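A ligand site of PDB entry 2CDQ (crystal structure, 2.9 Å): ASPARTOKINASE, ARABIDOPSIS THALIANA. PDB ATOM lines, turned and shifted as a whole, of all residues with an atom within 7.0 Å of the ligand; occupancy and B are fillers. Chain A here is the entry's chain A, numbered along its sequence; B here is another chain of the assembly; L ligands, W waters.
The backbone carbonyl oxygen of Ser 371 lies within hydrogen-bond range of a nitrogen (N4) of the ligand, 3.1 Å away.
The backbone NH of Arg 394 sits at hydrogen-bond distance from an oxygen (O5) of the ligand (3.1 Å).
N of Ser 371 sits at hydrogen-bond distance from N5 of the ligand, 2.8 Å away.
The backbone NH of Ser 393 is in hydrogen-bond range of an oxygen (O5) of the ligand (2.9 Å).
The guanidinium group (NH2) of Arg 394 sits close to an oxygen (O4) of the ligand (3.5 Å).
The side-chain hydroxyl (OG) of Ser 393 lies within hydrogen-bond range of an oxygen (O5) of the ligand, 2.7 Å away.
The side-chain carboxylate (OD2) of Asp 387 is in hydrogen-bond range of the side-chain hydroxyl (OG) of Ser 371 (2.5 Å).
The side-chain carboxylate (OD2) of Asp 387 is in hydrogen-bond range of the indole nitrogen (NE1) of Trp 392, at 3.3 Å.
The backbone NH (N) of Ile 397 sits at hydrogen-bond distance from the side-chain carboxylate (OE2) of Glu 400, at 3.3 Å.
The side-chain carboxylate (OE2) of Glu 400 lies within salt-bridge range of the guanidinium group (NH1) of Arg 394 (3.2 Å).
A sulfur (S1) of the ligand lies close to the backbone carbonyl oxygen (O) of Gly 369 (3.6 Å).
O of Leu 368 touches C5 of the ligand, 3.9 Å away.
CA of Ile 370 touches N5 of the ligand, 3.5 Å away.
Asp 387 touches the ligand.
Trp 392 touches the ligand.
CD2 of Leu 396 touches C11 of the ligand (3.5 Å).
Glu 400 touches the ligand.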
ATOM      1  N   GLU A 367      -1.031   0.653  25.088  1.00  0.00           N
ATOM      2  CA  GLU A 367      -0.205   1.820  24.811  1.00  0.00           C
ATOM      3  C   GLU A 367       1.247   1.602  25.214  1.00  0.00           C
ATOM      4  O   GLU A 367       2.145   2.245  24.673  1.00  0.00           O
ATOM      5  CB  GLU A 367      -0.784   3.074  25.493  1.00  0.00           C
ATOM      6  CG  GLU A 367      -2.033   3.639  24.813  1.00  0.00           C
ATOM      7  CD  GLU A 367      -1.785   4.006  23.352  1.00  0.00           C
ATOM      8  OE1 GLU A 367      -1.135   5.059  23.085  1.00  0.00           O
ATOM      9  OE2 GLU A 367      -2.233   3.253  22.452  1.00  0.00           O
ATOM     10  N   LEU A 368       1.476   0.690  26.169  1.00  0.00           N
ATOM     11  CA  LEU A 368       2.832   0.377  26.615  1.00  0.00           C
ATOM     12  C   LEU A 368       3.398  -0.902  26.006  1.00  0.00           C
ATOM     13  O   LEU A 368       4.457  -1.393  26.423  1.00  0.00           O
ATOM     14  CB  LEU A 368       2.901   0.350  28.148  1.00  0.00           C
ATOM     15  CG  LEU A 368       3.387   1.645  28.811  1.00  0.00           C
ATOM     16  CD1 LEU A 368       2.324   2.751  28.765  1.00  0.00           C
ATOM     17  CD2 LEU A 368       3.806   1.343  30.243  1.00  0.00           C
ATOM     18  N   GLY A 369       2.689  -1.427  25.002  1.00  0.00           N
ATOM     19  CA  GLY A 369       3.129  -2.579  24.208  1.00  0.00           C
ATOM     20  C   GLY A 369       3.296  -3.911  24.951  1.00  0.00           C
ATOM     21  O   GLY A 369       4.088  -4.758  24.524  1.00  0.00           O
ATOM     22  N   ILE A 370       2.542  -4.084  26.036  1.00  0.00           N
ATOM     23  CA  ILE A 370       2.651  -5.282  26.875  1.00  0.00           C
ATOM     24  C   ILE A 370       1.441  -6.222  26.711  1.00  0.00           C
ATOM     25  O   ILE A 370       0.285  -5.782  26.750  1.00  0.00           O
ATOM     26  CB  ILE A 370       2.825  -4.926  28.380  1.00  0.00           C
ATOM     27  CG1 ILE A 370       4.105  -4.119  28.606  1.00  0.00           C
ATOM     28  CG2 ILE A 370       2.860  -6.182  29.230  1.00  0.00           C
ATOM     29  CD1 ILE A 370       4.368  -3.772  30.057  1.00  0.00           C
ATOM     30  N   SER A 371       1.731  -7.508  26.532  1.00  0.00           N
ATOM     31  CA  SER A 371       0.707  -8.526  26.491  1.00  0.00           C
ATOM     32  C   SER A 371       0.509  -9.208  27.857  1.00  0.00           C
ATOM     33  O   SER A 371       1.459  -9.727  28.445  1.00  0.00           O
ATOM     34  CB  SER A 371       1.003  -9.567  25.405  1.00  0.00           C
ATOM     35  OG  SER A 371       0.069 -10.632  25.452  1.00  0.00           O
ATOM     36  N   VAL A 372      -0.734  -9.168  28.326  1.00  0.00           N
ATOM     37  CA  VAL A 372      -1.185  -9.756  29.585  1.00  0.00           C
ATOM     38  C   VAL A 372      -1.627 -11.199  29.337  1.00  0.00           C
ATOM     39  O   VAL A 372      -2.129 -11.521  28.268  1.00  0.00           O
ATOM     40  CB  VAL A 372      -2.404  -8.963  30.134  1.00  0.00           C
ATOM     41  CG1 VAL A 372      -2.844  -9.490  31.501  1.00  0.00           C
ATOM     42  CG2 VAL A 372      -2.092  -7.480  30.209  1.00  0.00           C
ATOM     43  N   ASP A 373      -1.431 -12.080  30.322  1.00  0.00           N
ATOM     44  CA  ASP A 373      -1.782 -13.496  30.180  1.00  0.00           C
ATOM     45  C   ASP A 373      -3.068 -13.849  30.936  1.00  0.00           C
ATOM     46  O   ASP A 373      -4.166 -13.826  30.374  1.00  0.00           O
ATOM     47  CB  ASP A 373      -0.603 -14.377  30.621  1.00  0.00           C
ATOM     48  CG  ASP A 373      -0.859 -15.869  30.417  1.00  0.00           C
ATOM     49  OD1 ASP A 373      -0.142 -16.667  31.048  1.00  0.00           O
ATOM     50  OD2 ASP A 373      -1.747 -16.257  29.627  1.00  0.00           O
ATOM     51  N   LEU A 386       1.509 -11.185  33.529  1.00  0.00           N
ATOM     52  CA  LEU A 386       2.064 -10.799  32.228  1.00  0.00           C
ATOM     53  C   LEU A 386       2.591 -12.014  31.476  1.00  0.00           C
ATOM     54  O   LEU A 386       3.111 -12.935  32.101  1.00  0.00           O
ATOM     55  CB  LEU A 386       3.186  -9.779  32.388  1.00  0.00           C
ATOM     56  CG  LEU A 386       2.818  -8.514  33.174  1.00  0.00           C
ATOM     57  CD1 LEU A 386       4.053  -7.697  33.473  1.00  0.00           C
ATOM     58  CD2 LEU A 386       1.794  -7.707  32.412  1.00  0.00           C
ATOM     59  N   ASP A 387       2.442 -12.020  30.157  1.00  0.00           N
ATOM     60  CA  ASP A 387       2.952 -13.120  29.320  1.00  0.00           C
ATOM     61  C   ASP A 387       4.297 -13.601  29.857  1.00  0.00           C
ATOM     62  O   ASP A 387       5.158 -12.786  30.197  1.00  0.00           O
ATOM     63  CB  ASP A 387       3.126 -12.660  27.875  1.00  0.00           C
ATOM     64  CG  ASP A 387       1.870 -12.824  27.028  1.00  0.00           C
ATOM     65  OD1 ASP A 387       0.879 -13.421  27.503  1.00  0.00           O
ATOM     66  OD2 ASP A 387       1.889 -12.352  25.879  1.00  0.00           O
ATOM     67  N   PRO A 388       4.499 -14.932  29.937  1.00  0.00           N
ATOM     68  CA  PRO A 388       5.800 -15.448  30.351  1.00  0.00           C
ATOM     69  C   PRO A 388       6.868 -14.960  29.377  1.00  0.00           C
ATOM     70  O   PRO A 388       6.591 -14.840  28.188  1.00  0.00           O
ATOM     71  CB  PRO A 388       5.636 -16.967  30.249  1.00  0.00           C
ATOM     72  CG  PRO A 388       4.170 -17.208  30.335  1.00  0.00           C
ATOM     73  CD  PRO A 388       3.539 -16.028  29.659  1.00  0.00           C
ATOM     74  N   SER A 389       8.063 -14.659  29.888  1.00  0.00           N
ATOM     75  CA  SER A 389       9.107 -14.047  29.072  1.00  0.00           C
ATOM     76  C   SER A 389       9.578 -14.900  27.886  1.00  0.00           C
ATOM     77  O   SER A 389       9.934 -14.349  26.835  1.00  0.00           O
ATOM     78  CB  SER A 389      10.312 -13.645  29.920  1.00  0.00           C
ATOM     79  OG  SER A 389      10.914 -14.800  30.481  1.00  0.00           O
ATOM     80  N   LEU A 391       7.979 -16.417  25.856  1.00  0.00           N
ATOM     81  CA  LEU A 391       7.066 -16.164  24.756  1.00  0.00           C
ATOM     82  C   LEU A 391       7.530 -14.965  23.937  1.00  0.00           C
ATOM     83  O   LEU A 391       6.991 -14.694  22.864  1.00  0.00           O
ATOM     84  CB  LEU A 391       5.676 -15.877  25.314  1.00  0.00           C
ATOM     85  CG  LEU A 391       4.443 -16.182  24.479  1.00  0.00           C
ATOM     86  CD1 LEU A 391       4.095 -17.644  24.650  1.00  0.00           C
ATOM     87  CD2 LEU A 391       3.308 -15.318  24.952  1.00  0.00           C
ATOM     88  N   TRP A 392       8.525 -14.257  24.465  1.00  0.00           N
ATOM     89  CA  TRP A 392       9.058 -13.042  23.843  1.00  0.00           C
ATOM     90  C   TRP A 392      10.575 -13.093  23.646  1.00  0.00           C
ATOM     91  O   TRP A 392      11.186 -14.155  23.804  1.00  0.00           O
ATOM     92  CB  TRP A 392       8.657 -11.823  24.673  1.00  0.00           C
ATOM     93  CG  TRP A 392       7.186 -11.596  24.670  1.00  0.00           C
ATOM     94  CD1 TRP A 392       6.281 -12.006  25.607  1.00  0.00           C
ATOM     95  CD2 TRP A 392       6.431 -10.916  23.653  1.00  0.00           C
ATOM     96  NE1 TRP A 392       5.017 -11.609  25.248  1.00  0.00           N
ATOM     97  CE2 TRP A 392       5.078 -10.944  24.057  1.00  0.00           C
ATOM     98  CE3 TRP A 392       6.764 -10.275  22.448  1.00  0.00           C
ATOM     99  CZ2 TRP A 392       4.050 -10.363  23.293  1.00  0.00           C
ATOM    100  CZ3 TRP A 392       5.749  -9.700  21.690  1.00  0.00           C
ATOM    101  CH2 TRP A 392       4.405  -9.746  22.130  1.00  0.00           C
ATOM    102  N   SER A 393      11.187 -11.962  23.303  1.00  0.00           N
ATOM    103  CA  SER A 393      12.609 -11.927  22.975  1.00  0.00           C
ATOM    104  C   SER A 393      13.482 -11.566  24.176  1.00  0.00           C
ATOM    105  O   SER A 393      14.681 -11.868  24.200  1.00  0.00           O
ATOM    106  CB  SER A 393      12.859 -10.932  21.832  1.00  0.00           C
ATOM    107  OG  SER A 393      12.690  -9.594  22.275  1.00  0.00           O
ATOM    108  N   ARG A 394      12.876 -10.942  25.168  1.00  0.00           N
ATOM    109  CA  ARG A 394      13.595 -10.392  26.306  1.00  0.00           C
ATOM    110  C   ARG A 394      12.663 -10.396  27.526  1.00  0.00           C
ATOM    111  O   ARG A 394      11.450 -10.587  27.385  1.00  0.00           O
ATOM    112  CB  ARG A 394      14.066  -8.972  25.952  1.00  0.00           C
ATOM    113  CG  ARG A 394      14.479  -8.091  27.113  1.00  0.00           C
ATOM    114  CD  ARG A 394      15.051  -6.738  26.676  1.00  0.00           C
ATOM    115  NE  ARG A 394      14.179  -5.949  25.802  1.00  0.00           N
ATOM    116  CZ  ARG A 394      13.132  -5.213  26.213  1.00  0.00           C
ATOM    117  NH1 ARG A 394      12.791  -5.164  27.504  1.00  0.00           N
ATOM    118  NH2 ARG A 394      12.433  -4.526  25.320  1.00  0.00           N
ATOM    119  N   GLU A 395      13.234 -10.234  28.705  1.00  0.00           N
ATOM    120  CA  GLU A 395      12.442  -9.946  29.896  1.00  0.00           C
ATOM    121  C   GLU A 395      12.173  -8.449  29.945  1.00  0.00           C
ATOM    122  O   GLU A 395      12.995  -7.662  29.477  1.00  0.00           O
ATOM    123  CB  GLU A 395      13.178 -10.371  31.156  1.00  0.00           C
ATOM    124  CG  GLU A 395      13.272 -11.872  31.317  1.00  0.00           C
ATOM    125  CD  GLU A 395      13.821 -12.296  32.674  1.00  0.00           C
ATOM    126  OE1 GLU A 395      14.648 -11.559  33.267  1.00  0.00           O
ATOM    127  OE2 GLU A 395      13.412 -13.373  33.146  1.00  0.00           O
ATOM    128  N   LEU A 396      11.021  -8.063  30.490  1.00  0.00           N
ATOM    129  CA  LEU A 396      10.740  -6.644  30.709  1.00  0.00           C
ATOM    130  C   LEU A 396      11.725  -6.083  31.737  1.00  0.00           C
ATOM    131  O   LEU A 396      11.965  -6.714  32.769  1.00  0.00           O
ATOM    132  CB  LEU A 396       9.295  -6.458  31.197  1.00  0.00           C
ATOM    133  CG  LEU A 396       8.164  -6.916  30.278  1.00  0.00           C
ATOM    134  CD1 LEU A 396       6.826  -6.899  31.024  1.00  0.00           C
ATOM    135  CD2 LEU A 396       8.087  -6.057  29.029  1.00  0.00           C
ATOM    136  N   ILE A 397      12.310  -4.924  31.442  1.00  0.00           N
ATOM    137  CA  ILE A 397      13.279  -4.299  32.349  1.00  0.00           C
ATOM    138  C   ILE A 397      12.598  -3.435  33.416  1.00  0.00           C
ATOM    139  O   ILE A 397      11.505  -2.896  33.197  1.00  0.00           O
ATOM    140  CB  ILE A 397      14.365  -3.483  31.592  1.00  0.00           C
ATOM    141  CG1 ILE A 397      13.740  -2.530  30.565  1.00  0.00           C
ATOM    142  CG2 ILE A 397      15.393  -4.426  30.941  1.00  0.00           C
ATOM    143  CD1 ILE A 397      14.548  -1.279  30.282  1.00  0.00           C
ATOM    144  N   GLN A 399      12.672  -0.531  34.444  1.00  0.00           N
ATOM    145  CA  GLN A 399      12.138   0.752  33.956  1.00  0.00           C
ATOM    146  C   GLN A 399      10.724   0.569  33.398  1.00  0.00           C
ATOM    147  O   GLN A 399       9.800   1.301  33.777  1.00  0.00           O
ATOM    148  CB  GLN A 399      13.073   1.359  32.895  1.00  0.00           C
ATOM    149  CG  GLN A 399      12.782   2.831  32.544  1.00  0.00           C
ATOM    150  CD  GLN A 399      11.435   3.028  31.817  1.00  0.00           C
ATOM    151  OE1 GLN A 399      11.160   2.378  30.807  1.00  0.00           O
ATOM    152  NE2 GLN A 399      10.618   3.940  32.345  1.00  0.00           N
ATOM    153  N   GLU A 400      10.563  -0.412  32.505  1.00  0.00           N
ATOM    154  CA  GLU A 400       9.287  -0.673  31.826  1.00  0.00           C
ATOM    155  C   GLU A 400       8.166  -0.998  32.804  1.00  0.00           C
ATOM    156  O   GLU A 400       7.028  -0.572  32.605  1.00  0.00           O
ATOM    157  CB  GLU A 400       9.432  -1.775  30.787  1.00  0.00           C
ATOM    158  CG  GLU A 400      10.332  -1.406  29.635  1.00  0.00           C
ATOM    159  CD  GLU A 400      10.543  -2.541  28.642  1.00  0.00           C
ATOM    160  OE1 GLU A 400      10.831  -2.221  27.471  1.00  0.00           O
ATOM    161  OE2 GLU A 400      10.422  -3.726  29.020  1.00  0.00           O
ATOM    162  N   GLY B 353      -0.306 -14.309  23.033  1.00  0.00           N
ATOM    163  CA  GLY B 353       0.864 -13.542  22.614  1.00  0.00           C
ATOM    164  C   GLY B 353       0.612 -12.239  21.861  1.00  0.00           C
ATOM    165  O   GLY B 353       1.554 -11.639  21.349  1.00  0.00           O
ATOM    166  N   VAL B 355      -0.753  -8.213  21.804  1.00  0.00           N
ATOM    167  CA  VAL B 355      -0.977  -7.024  22.642  1.00  0.00           C
ATOM    168  C   VAL B 355      -2.270  -6.345  22.189  1.00  0.00           C
ATOM    169  O   VAL B 355      -2.501  -6.189  20.994  1.00  0.00           O
ATOM    170  CB  VAL B 355       0.214  -6.013  22.515  1.00  0.00           C
ATOM    171  CG1 VAL B 355      -0.006  -4.785  23.382  1.00  0.00           C
ATOM    172  CG2 VAL B 355       1.532  -6.683  22.885  1.00  0.00           C
HETATM  173  N1  LIG L   1       8.776   1.175  25.563  1.00  0.00           N
HETATM  174  C1  LIG L   1       8.879   0.007  24.696  1.00  0.00           C
HETATM  175  C2  LIG L   1       8.023   0.134  23.436  1.00  0.00           C
HETATM  176  O1  LIG L   1       8.430  -0.277  22.337  1.00  0.00           O
HETATM  177  O2  LIG L   1       6.899   0.638  23.469  1.00  0.00           O
HETATM  178  C3  LIG L   1       8.517  -1.261  25.462  1.00  0.00           C
HETATM  179  C4  LIG L   1       8.961  -2.572  24.812  1.00  0.00           C
HETATM  180  S1  LIG L   1       7.555  -3.633  24.404  1.00  0.00           S
HETATM  181  C5  LIG L   1       7.076  -4.238  26.037  1.00  0.00           C
HETATM  182  C6  LIG L   1       8.222  -5.090  23.543  1.00  0.00           C
HETATM  183  C7  LIG L   1       9.498  -5.748  24.071  1.00  0.00           C
HETATM  184  O3  LIG L   1       9.331  -6.252  25.383  1.00  0.00           O
HETATM  185  C8  LIG L   1       9.912  -6.938  23.223  1.00  0.00           C
HETATM  186  O4  LIG L   1      11.300  -6.855  22.984  1.00  0.00           O
HETATM  187  C9  LIG L   1       9.621  -8.177  24.048  1.00  0.00           C
HETATM  188  O5  LIG L   1      10.653  -9.145  23.932  1.00  0.00           O
HETATM  189  C10 LIG L   1       9.558  -7.648  25.471  1.00  0.00           C
HETATM  190  N2  LIG L   1       8.506  -8.290  26.293  1.00  0.00           N
HETATM  191  C11 LIG L   1       8.714  -9.077  27.384  1.00  0.00           C
HETATM  192  N3  LIG L   1       7.528  -9.447  27.906  1.00  0.00           N
HETATM  193  C12 LIG L   1       6.553  -8.901  27.160  1.00  0.00           C
HETATM  194  C13 LIG L   1       5.162  -8.966  27.242  1.00  0.00           C
HETATM  195  N4  LIG L   1       4.564  -9.657  28.199  1.00  0.00           N
HETATM  196  N5  LIG L   1       4.397  -8.280  26.305  1.00  0.00           N
HETATM  197  C14 LIG L   1       5.014  -7.549  25.308  1.00  0.00           C
HETATM  198  N6  LIG L   1       6.393  -7.502  25.237  1.00  0.00           N
HETATM  199  C15 LIG L   1       7.144  -8.157  26.142  1.00  0.00           C
HETATM  200  O   HOH W   1      11.421  -2.665  22.555  1.00  0.00           O
